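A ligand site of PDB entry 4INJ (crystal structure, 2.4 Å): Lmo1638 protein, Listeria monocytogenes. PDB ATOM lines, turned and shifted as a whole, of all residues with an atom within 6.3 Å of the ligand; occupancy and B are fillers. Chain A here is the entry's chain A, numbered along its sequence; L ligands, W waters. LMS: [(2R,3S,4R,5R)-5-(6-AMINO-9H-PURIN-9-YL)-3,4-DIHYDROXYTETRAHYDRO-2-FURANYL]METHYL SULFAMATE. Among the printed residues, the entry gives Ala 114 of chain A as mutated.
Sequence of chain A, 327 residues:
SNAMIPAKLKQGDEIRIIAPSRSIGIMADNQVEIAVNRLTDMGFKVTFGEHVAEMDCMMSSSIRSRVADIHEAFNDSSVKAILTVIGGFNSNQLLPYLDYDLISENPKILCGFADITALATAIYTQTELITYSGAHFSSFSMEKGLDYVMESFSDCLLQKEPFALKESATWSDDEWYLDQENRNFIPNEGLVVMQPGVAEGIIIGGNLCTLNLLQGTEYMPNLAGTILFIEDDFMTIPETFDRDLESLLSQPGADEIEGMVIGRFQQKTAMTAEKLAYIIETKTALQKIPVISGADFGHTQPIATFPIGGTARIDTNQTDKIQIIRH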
ATOM      1  N   ARG A  22     -25.927 -31.452   1.551  1.00  0.00           N
ATOM      2  CA  ARG A  22     -25.891 -32.706   0.812  1.00  0.00           C
ATOM      3  C   ARG A  22     -25.172 -33.806   1.601  1.00  0.00           C
ATOM      4  O   ARG A  22     -24.374 -33.538   2.520  1.00  0.00           O
ATOM      5  CB  ARG A  22     -25.236 -32.505  -0.550  1.00  0.00           C
ATOM      6  CG  ARG A  22     -26.183 -31.957  -1.595  1.00  0.00           C
ATOM      7  CD  ARG A  22     -25.546 -31.759  -2.944  1.00  0.00           C
ATOM      8  NE  ARG A  22     -24.407 -30.839  -2.901  1.00  0.00           N
ATOM      9  CZ  ARG A  22     -23.579 -30.595  -3.913  1.00  0.00           C
ATOM     10  NH1 ARG A  22     -23.717 -31.248  -5.050  1.00  0.00           N
ATOM     11  NH2 ARG A  22     -22.588 -29.720  -3.763  1.00  0.00           N
ATOM     12  N   ILE A  26     -22.141 -38.315  -1.549  1.00  0.00           N
ATOM     13  CA  ILE A  26     -21.711 -37.829  -2.841  1.00  0.00           C
ATOM     14  C   ILE A  26     -20.191 -37.805  -2.847  1.00  0.00           C
ATOM     15  O   ILE A  26     -19.628 -37.606  -3.903  1.00  0.00           O
ATOM     16  CB  ILE A  26     -22.284 -36.433  -3.226  1.00  0.00           C
ATOM     17  CG1 ILE A  26     -21.785 -35.368  -2.261  1.00  0.00           C
ATOM     18  CG2 ILE A  26     -23.803 -36.471  -3.264  1.00  0.00           C
ATOM     19  CD1 ILE A  26     -21.878 -33.958  -2.793  1.00  0.00           C
ATOM     20  N   MET A  27     -19.543 -37.946  -1.670  1.00  0.00           N
ATOM     21  CA  MET A  27     -18.075 -38.032  -1.612  1.00  0.00           C
ATOM     22  C   MET A  27     -17.713 -39.502  -1.792  1.00  0.00           C
ATOM     23  O   MET A  27     -18.347 -40.332  -1.213  1.00  0.00           O
ATOM     24  CB  MET A  27     -17.512 -37.558  -0.282  1.00  0.00           C
ATOM     25  CG  MET A  27     -17.721 -36.107   0.102  1.00  0.00           C
ATOM     26  SD  MET A  27     -16.903 -35.858   1.707  1.00  0.00           S
ATOM     27  CE  MET A  27     -15.157 -35.786   1.309  1.00  0.00           C
ATOM     28  N   ALA A  28     -16.715 -39.801  -2.625  1.00  0.00           N
ATOM     29  CA  ALA A  28     -16.250 -41.167  -2.818  1.00  0.00           C
ATOM     30  C   ALA A  28     -15.491 -41.646  -1.593  1.00  0.00           C
ATOM     31  O   ALA A  28     -14.885 -40.825  -0.858  1.00  0.00           O
ATOM     32  CB  ALA A  28     -15.365 -41.265  -4.054  1.00  0.00           C
ATOM     33  N   GLN A  31     -12.210 -40.099  -1.014  1.00  0.00           N
ATOM     34  CA  GLN A  31     -12.126 -38.677  -0.573  1.00  0.00           C
ATOM     35  C   GLN A  31     -12.300 -38.585   0.944  1.00  0.00           C
ATOM     36  O   GLN A  31     -11.550 -37.881   1.651  1.00  0.00           O
ATOM     37  CB  GLN A  31     -13.219 -37.837  -1.189  1.00  0.00           C
ATOM     38  CG  GLN A  31     -13.086 -37.427  -2.642  1.00  0.00           C
ATOM     39  CD  GLN A  31     -14.270 -36.538  -3.045  1.00  0.00           C
ATOM     40  OE1 GLN A  31     -15.189 -36.978  -3.753  1.00  0.00           O
ATOM     41  NE2 GLN A  31     -14.276 -35.303  -2.553  1.00  0.00           N
ATOM     42  N   ILE A  86     -20.269 -30.764   3.161  1.00  0.00           N
ATOM     43  CA  ILE A  86     -20.300 -30.124   1.888  1.00  0.00           C
ATOM     44  C   ILE A  86     -21.553 -29.214   1.854  1.00  0.00           C
ATOM     45  O   ILE A  86     -22.448 -29.362   2.685  1.00  0.00           O
ATOM     46  CB  ILE A  86     -20.364 -31.184   0.755  1.00  0.00           C
ATOM     47  CG1 ILE A  86     -20.026 -30.608  -0.611  1.00  0.00           C
ATOM     48  CG2 ILE A  86     -21.715 -31.843   0.661  1.00  0.00           C
ATOM     49  CD1 ILE A  86     -18.569 -30.199  -0.718  1.00  0.00           C
ATOM     50  N   GLY A  87     -21.606 -28.301   0.888  1.00  0.00           N
ATOM     51  CA  GLY A  87     -22.770 -27.468   0.632  1.00  0.00           C
ATOM     52  C   GLY A  87     -23.825 -28.202  -0.118  1.00  0.00           C
ATOM     53  O   GLY A  87     -23.959 -29.382   0.008  1.00  0.00           O
ATOM     54  N   GLY A  88     -24.589 -27.495  -0.932  1.00  0.00           N
ATOM     55  CA  GLY A  88     -25.823 -28.041  -1.458  1.00  0.00           C
ATOM     56  C   GLY A  88     -26.864 -26.920  -1.585  1.00  0.00           C
ATOM     57  O   GLY A  88     -26.635 -25.928  -2.206  1.00  0.00           O
ATOM     58  N   PHE A 113     -19.172 -23.551   4.223  1.00  0.00           N
ATOM     59  CA  PHE A 113     -19.452 -22.363   3.410  1.00  0.00           C
ATOM     60  C   PHE A 113     -20.520 -22.653   2.385  1.00  0.00           C
ATOM     61  O   PHE A 113     -21.075 -23.746   2.342  1.00  0.00           O
ATOM     62  CB  PHE A 113     -18.144 -21.712   2.808  1.00  0.00           C
ATOM     63  CG  PHE A 113     -17.592 -22.412   1.619  1.00  0.00           C
ATOM     64  CD1 PHE A 113     -16.825 -23.542   1.763  1.00  0.00           C
ATOM     65  CD2 PHE A 113     -17.821 -21.950   0.338  1.00  0.00           C
ATOM     66  CE1 PHE A 113     -16.324 -24.218   0.652  1.00  0.00           C
ATOM     67  CE2 PHE A 113     -17.346 -22.612  -0.792  1.00  0.00           C
ATOM     68  CZ  PHE A 113     -16.579 -23.731  -0.628  1.00  0.00           C
ATOM     69  N   ALA A 114     -20.789 -21.645   1.562  1.00  0.00           N
ATOM     70  CA  ALA A 114     -21.796 -21.750   0.504  1.00  0.00           C
ATOM     71  C   ALA A 114     -23.169 -21.966   1.130  1.00  0.00           C
ATOM     72  O   ALA A 114     -23.619 -21.133   1.861  1.00  0.00           O
ATOM     73  CB  ALA A 114     -21.427 -22.849  -0.493  1.00  0.00           C
ATOM     74  N   ASP A 115     -23.834 -23.080   0.880  1.00  0.00           N
ATOM     75  CA  ASP A 115     -25.165 -23.246   1.379  1.00  0.00           C
ATOM     76  C   ASP A 115     -25.266 -23.105   2.906  1.00  0.00           C
ATOM     77  O   ASP A 115     -26.306 -22.731   3.466  1.00  0.00           O
ATOM     78  CB  ASP A 115     -25.784 -24.587   0.962  1.00  0.00           C
ATOM     79  CG  ASP A 115     -27.270 -24.701   1.455  1.00  0.00           C
ATOM     80  OD1 ASP A 115     -28.132 -23.931   0.939  1.00  0.00           O
ATOM     81  OD2 ASP A 115     -27.525 -25.484   2.394  1.00  0.00           O
ATOM     82  N   HIS A 136     -15.236 -26.714   4.514  1.00  0.00           N
ATOM     83  CA  HIS A 136     -15.932 -27.977   4.744  1.00  0.00           C
ATOM     84  C   HIS A 136     -14.983 -29.101   5.177  1.00  0.00           C
ATOM     85  O   HIS A 136     -13.814 -28.970   5.079  1.00  0.00           O
ATOM     86  CB  HIS A 136     -16.550 -28.464   3.426  1.00  0.00           C
ATOM     87  CG  HIS A 136     -17.698 -27.639   2.937  1.00  0.00           C
ATOM     88  ND1 HIS A 136     -18.797 -27.324   3.728  1.00  0.00           N
ATOM     89  CD2 HIS A 136     -17.939 -27.088   1.728  1.00  0.00           C
ATOM     90  CE1 HIS A 136     -19.645 -26.603   3.029  1.00  0.00           C
ATOM     91  NE2 HIS A 136     -19.153 -26.435   1.814  1.00  0.00           N
ATOM     92  N   SER A 138     -14.951 -31.866   3.531  1.00  0.00           N
ATOM     93  CA  SER A 138     -14.528 -32.241   2.171  1.00  0.00           C
ATOM     94  C   SER A 138     -13.443 -31.329   1.577  1.00  0.00           C
ATOM     95  O   SER A 138     -12.733 -31.732   0.656  1.00  0.00           O
ATOM     96  CB  SER A 138     -15.737 -32.259   1.241  1.00  0.00           C
ATOM     97  OG  SER A 138     -16.251 -30.927   1.111  1.00  0.00           O
ATOM     98  N   SER A 139     -13.290 -30.110   2.116  1.00  0.00           N
ATOM     99  CA  SER A 139     -12.256 -29.235   1.671  1.00  0.00           C
ATOM    100  C   SER A 139     -10.858 -29.791   1.950  1.00  0.00           C
ATOM    101  O   SER A 139      -9.926 -29.517   1.181  1.00  0.00           O
ATOM    102  CB  SER A 139     -12.397 -27.884   2.327  1.00  0.00           C
ATOM    103  OG  SER A 139     -13.645 -27.311   1.994  1.00  0.00           O
ATOM    104  N   SER A 141      -9.916 -32.763   1.715  1.00  0.00           N
ATOM    105  CA  SER A 141      -9.552 -33.866   0.850  1.00  0.00           C
ATOM    106  C   SER A 141      -8.810 -33.397  -0.402  1.00  0.00           C
ATOM    107  O   SER A 141      -8.598 -34.185  -1.317  1.00  0.00           O
ATOM    108  CB  SER A 141     -10.796 -34.678   0.464  1.00  0.00           C
ATOM    109  OG  SER A 141     -11.590 -34.016  -0.449  1.00  0.00           O
ATOM    110  N   ASP A 174     -10.536 -25.486 -10.295  1.00  0.00           N
ATOM    111  CA  ASP A 174     -10.509 -26.845 -10.896  1.00  0.00           C
ATOM    112  C   ASP A 174     -11.490 -27.752 -10.184  1.00  0.00           C
ATOM    113  O   ASP A 174     -11.787 -27.546  -9.003  1.00  0.00           O
ATOM    114  CB  ASP A 174      -9.095 -27.458 -10.874  1.00  0.00           C
ATOM    115  CG  ASP A 174      -8.002 -26.453 -11.207  1.00  0.00           C
ATOM    116  OD1 ASP A 174      -8.144 -25.673 -12.191  1.00  0.00           O
ATOM    117  OD2 ASP A 174      -7.005 -26.405 -10.467  1.00  0.00           O
ATOM    118  N   GLU A 175     -12.008 -28.720 -10.926  1.00  0.00           N
ATOM    119  CA  GLU A 175     -12.824 -29.780 -10.360  1.00  0.00           C
ATOM    120  C   GLU A 175     -11.839 -30.818  -9.816  1.00  0.00           C
ATOM    121  O   GLU A 175     -11.693 -31.927 -10.354  1.00  0.00           O
ATOM    122  CB  GLU A 175     -13.752 -30.392 -11.387  1.00  0.00           C
ATOM    123  CG  GLU A 175     -14.944 -29.506 -11.695  1.00  0.00           C
ATOM    124  CD  GLU A 175     -15.699 -29.986 -12.915  1.00  0.00           C
ATOM    125  OE1 GLU A 175     -15.104 -30.730 -13.737  1.00  0.00           O
ATOM    126  OE2 GLU A 175     -16.876 -29.611 -13.065  1.00  0.00           O
ATOM    127  N   TRP A 176     -11.144 -30.433  -8.764  1.00  0.00           N
ATOM    128  CA  TRP A 176     -10.088 -31.246  -8.205  1.00  0.00           C
ATOM    129  C   TRP A 176     -10.525 -32.577  -7.550  1.00  0.00           C
ATOM    130  O   TRP A 176      -9.708 -33.484  -7.415  1.00  0.00           O
ATOM    131  CB  TRP A 176      -9.321 -30.412  -7.212  1.00  0.00           C
ATOM    132  CG  TRP A 176     -10.158 -29.846  -6.082  1.00  0.00           C
ATOM    133  CD1 TRP A 176     -10.650 -28.585  -5.994  1.00  0.00           C
ATOM    134  CD2 TRP A 176     -10.569 -30.509  -4.894  1.00  0.00           C
ATOM    135  NE1 TRP A 176     -11.329 -28.410  -4.826  1.00  0.00           N
ATOM    136  CE2 TRP A 176     -11.299 -29.579  -4.124  1.00  0.00           C
ATOM    137  CE3 TRP A 176     -10.362 -31.802  -4.387  1.00  0.00           C
ATOM    138  CZ2 TRP A 176     -11.838 -29.905  -2.886  1.00  0.00           C
ATOM    139  CZ3 TRP A 176     -10.906 -32.121  -3.137  1.00  0.00           C
ATOM    140  CH2 TRP A 176     -11.638 -31.180  -2.410  1.00  0.00           C
ATOM    141  N   TYR A 177     -11.775 -32.690  -7.112  1.00  0.00           N
ATOM    142  CA  TYR A 177     -12.229 -33.933  -6.507  1.00  0.00           C
ATOM    143  C   TYR A 177     -12.292 -35.018  -7.564  1.00  0.00           C
ATOM    144  O   TYR A 177     -12.228 -36.208  -7.212  1.00  0.00           O
ATOM    145  CB  TYR A 177     -13.628 -33.791  -5.785  1.00  0.00           C
ATOM    146  CG  TYR A 177     -14.792 -33.393  -6.652  1.00  0.00           C
ATOM    147  CD1 TYR A 177     -14.963 -32.043  -7.056  1.00  0.00           C
ATOM    148  CD2 TYR A 177     -15.714 -34.338  -7.055  1.00  0.00           C
ATOM    149  CE1 TYR A 177     -16.014 -31.689  -7.886  1.00  0.00           C
ATOM    150  CE2 TYR A 177     -16.778 -33.983  -7.865  1.00  0.00           C
ATOM    151  CZ  TYR A 177     -16.920 -32.665  -8.282  1.00  0.00           C
ATOM    152  OH  TYR A 177     -18.004 -32.350  -9.084  1.00  0.00           O
ATOM    153  N   ASP A 233     -21.148 -18.661  -6.689  1.00  0.00           N
ATOM    154  CA  ASP A 233     -20.498 -19.717  -7.484  1.00  0.00           C
ATOM    155  C   ASP A 233     -20.759 -19.574  -8.978  1.00  0.00           C
ATOM    156  O   ASP A 233     -21.275 -18.574  -9.380  1.00  0.00           O
ATOM    157  CB  ASP A 233     -20.905 -21.114  -6.960  1.00  0.00           C
ATOM    158  CG  ASP A 233     -22.278 -21.522  -7.320  1.00  0.00           C
ATOM    159  OD1 ASP A 233     -23.025 -20.831  -8.020  1.00  0.00           O
ATOM    160  OD2 ASP A 233     -22.658 -22.602  -6.846  1.00  0.00           O
ATOM    161  N   GLN A 266     -15.775 -17.666  -9.959  1.00  0.00           N
ATOM    162  CA  GLN A 266     -15.381 -18.750 -10.788  1.00  0.00           C
ATOM    163  C   GLN A 266     -15.312 -18.244 -12.220  1.00  0.00           C
ATOM    164  O   GLN A 266     -15.874 -17.185 -12.528  1.00  0.00           O
ATOM    165  CB  GLN A 266     -16.359 -19.928 -10.601  1.00  0.00           C
ATOM    166  CG  GLN A 266     -16.243 -20.578  -9.217  1.00  0.00           C
ATOM    167  CD  GLN A 266     -16.910 -21.910  -9.144  1.00  0.00           C
ATOM    168  OE1 GLN A 266     -18.073 -22.063  -8.707  1.00  0.00           O
ATOM    169  NE2 GLN A 266     -16.202 -22.906  -9.611  1.00  0.00           N
ATOM    170  N   HIS A 299     -15.873 -19.926  -4.174  1.00  0.00           N
ATOM    171  CA  HIS A 299     -15.763 -21.231  -4.774  1.00  0.00           C
ATOM    172  C   HIS A 299     -14.477 -21.483  -5.616  1.00  0.00           C
ATOM    173  O   HIS A 299     -14.404 -22.467  -6.346  1.00  0.00           O
ATOM    174  CB  HIS A 299     -16.977 -21.497  -5.592  1.00  0.00           C
ATOM    175  CG  HIS A 299     -18.168 -21.818  -4.768  1.00  0.00           C
ATOM    176  ND1 HIS A 299     -18.957 -20.840  -4.182  1.00  0.00           N
ATOM    177  CD2 HIS A 299     -18.735 -23.005  -4.436  1.00  0.00           C
ATOM    178  CE1 HIS A 299     -19.929 -21.417  -3.517  1.00  0.00           C
ATOM    179  NE2 HIS A 299     -19.831 -22.725  -3.666  1.00  0.00           N
ATOM    180  N   GLN A 301     -10.202 -22.133  -5.510  1.00  0.00           N
ATOM    181  CA  GLN A 301      -9.157 -22.521  -4.558  1.00  0.00           C
ATOM    182  C   GLN A 301      -8.084 -21.494  -4.537  1.00  0.00           C
ATOM    183  O   GLN A 301      -7.716 -20.994  -5.573  1.00  0.00           O
ATOM    184  CB  GLN A 301      -8.571 -23.841  -4.957  1.00  0.00           C
ATOM    185  CG  GLN A 301      -9.618 -24.921  -5.128  1.00  0.00           C
ATOM    186  CD  GLN A 301     -10.225 -24.944  -6.503  1.00  0.00           C
ATOM    187  OE1 GLN A 301      -9.559 -24.696  -7.504  1.00  0.00           O
ATOM    188  NE2 GLN A 301     -11.481 -25.305  -6.573  1.00  0.00           N
HETATM  189  N9  LMS L   1     -16.429 -30.816  -4.115  1.00  0.00           N
HETATM  190  C8  LMS L   1     -15.621 -31.635  -3.390  1.00  0.00           C
HETATM  191  N7  LMS L   1     -16.103 -32.912  -3.424  1.00  0.00           N
HETATM  192  C5  LMS L   1     -17.214 -32.903  -4.157  1.00  0.00           C
HETATM  193  C6  LMS L   1     -18.188 -33.913  -4.559  1.00  0.00           C
HETATM  194  N6  LMS L   1     -17.986 -35.159  -4.152  1.00  0.00           N
HETATM  195  N1  LMS L   1     -19.277 -33.549  -5.297  1.00  0.00           N
HETATM  196  C2  LMS L   1     -19.426 -32.259  -5.682  1.00  0.00           C
HETATM  197  N3  LMS L   1     -18.544 -31.254  -5.340  1.00  0.00           N
HETATM  198  C4  LMS L   1     -17.447 -31.531  -4.591  1.00  0.00           C
HETATM  199  N   LMS L   1     -21.284 -25.399  -2.913  1.00  0.00           N
HETATM  200  S   LMS L   1     -20.467 -26.514  -2.120  1.00  0.00           S
HETATM  201  O1P LMS L   1     -20.151 -26.048  -0.788  1.00  0.00           O
HETATM  202  O2P LMS L   1     -21.118 -27.810  -2.202  1.00  0.00           O
HETATM  203  O5' LMS L   1     -19.044 -26.572  -2.674  1.00  0.00           O
HETATM  204  C5' LMS L   1     -18.900 -27.222  -3.919  1.00  0.00           C
HETATM  205  C4' LMS L   1     -17.403 -27.409  -4.050  1.00  0.00           C
HETATM  206  O4' LMS L   1     -17.014 -28.620  -3.424  1.00  0.00           O
HETATM  207  C3' LMS L   1     -17.023 -27.446  -5.509  1.00  0.00           C
HETATM  208  O3' LMS L   1     -16.013 -26.429  -5.612  1.00  0.00           O
HETATM  209  C2' LMS L   1     -16.535 -28.844  -5.735  1.00  0.00           C
HETATM  210  O2' LMS L   1     -15.363 -28.799  -6.575  1.00  0.00           O
HETATM  211  C1' LMS L   1     -16.219 -29.355  -4.310  1.00  0.00           C
HETATM  212  O   HOH W   1     -23.378 -24.920  -1.381  1.00  0.00           O
HETATM  213  O   HOH W   2     -16.645 -38.008  -5.412  1.00  0.00           O
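CA of Met 27 touches N6 of the ligand (3.8 Å).
CG1 of Ile 86 touches O2P of the ligand (3.4 Å).
Gly 88 touches the ligand (N to O2P, 3.7 Å).
Phe 113 touches the ligand (O to O1P, 3.99 Å).
Ala 114 touches the ligand (CB to O1P, 3.5 Å).
Tyr 177 touches the ligand.
Hydrophobic or aromatic side chains that line the ligand: Ile 26, Ile 86, Ala 114, His 136, Tyr 177 and His 299.
The nearest printed residue that does not touch the ligand is Trp 176 (4.1 Å).
OE1 of Gln 31 is in hydrogen-bond range of N of Ala 28 (3.4 Å).
The backbone carbonyl oxygen (O) of Gly 87 sits at hydrogen-bond distance from the backbone NH (N) of Arg 22 (3.2 Å).
The side-chain hydroxyl (OG) of Ser 139 lies within hydrogen-bond range of the backbone NH (N) of His 136 (3.0 Å).
A ring nitrogen (NE2) of His 136 lies within hydrogen-bond range of the backbone NH (N) of Gly 87, 3.2 Å away.
NE2 of His 136 lies close to O of Phe 113, 3.3 Å away.
Water W2 lies within hydrogen-bond range of OE1 of Gln 31 (2.4 Å), N of Ala 28 (3.3 Å), O of Ile 26 (3.4 Å) and N6 of the ligand (3.4 Å).
The backbone NH (N) of Gly 87 lies within hydrogen-bond range of an oxygen (O1P) of the ligand, 3.2 Å away.
NE2 of Gln 31 lies within hydrogen-bond range of N7 of the ligand (3.1 Å).
NE2 of His 136 lies within hydrogen-bond range of O1P of the ligand (2.8 Å).
O2P of the ligand is in hydrogen-bond range of NH2 of Arg 22, 2.9 Å away.
A ring nitrogen (NE2) of His 299 sits at hydrogen-bond distance from a nitrogen (N) of the ligand (3.1 Å).
The backbone carbonyl oxygen (O) of Ile 26 is in hydrogen-bond range of a nitrogen (N6) of the ligand (3.0 Å).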
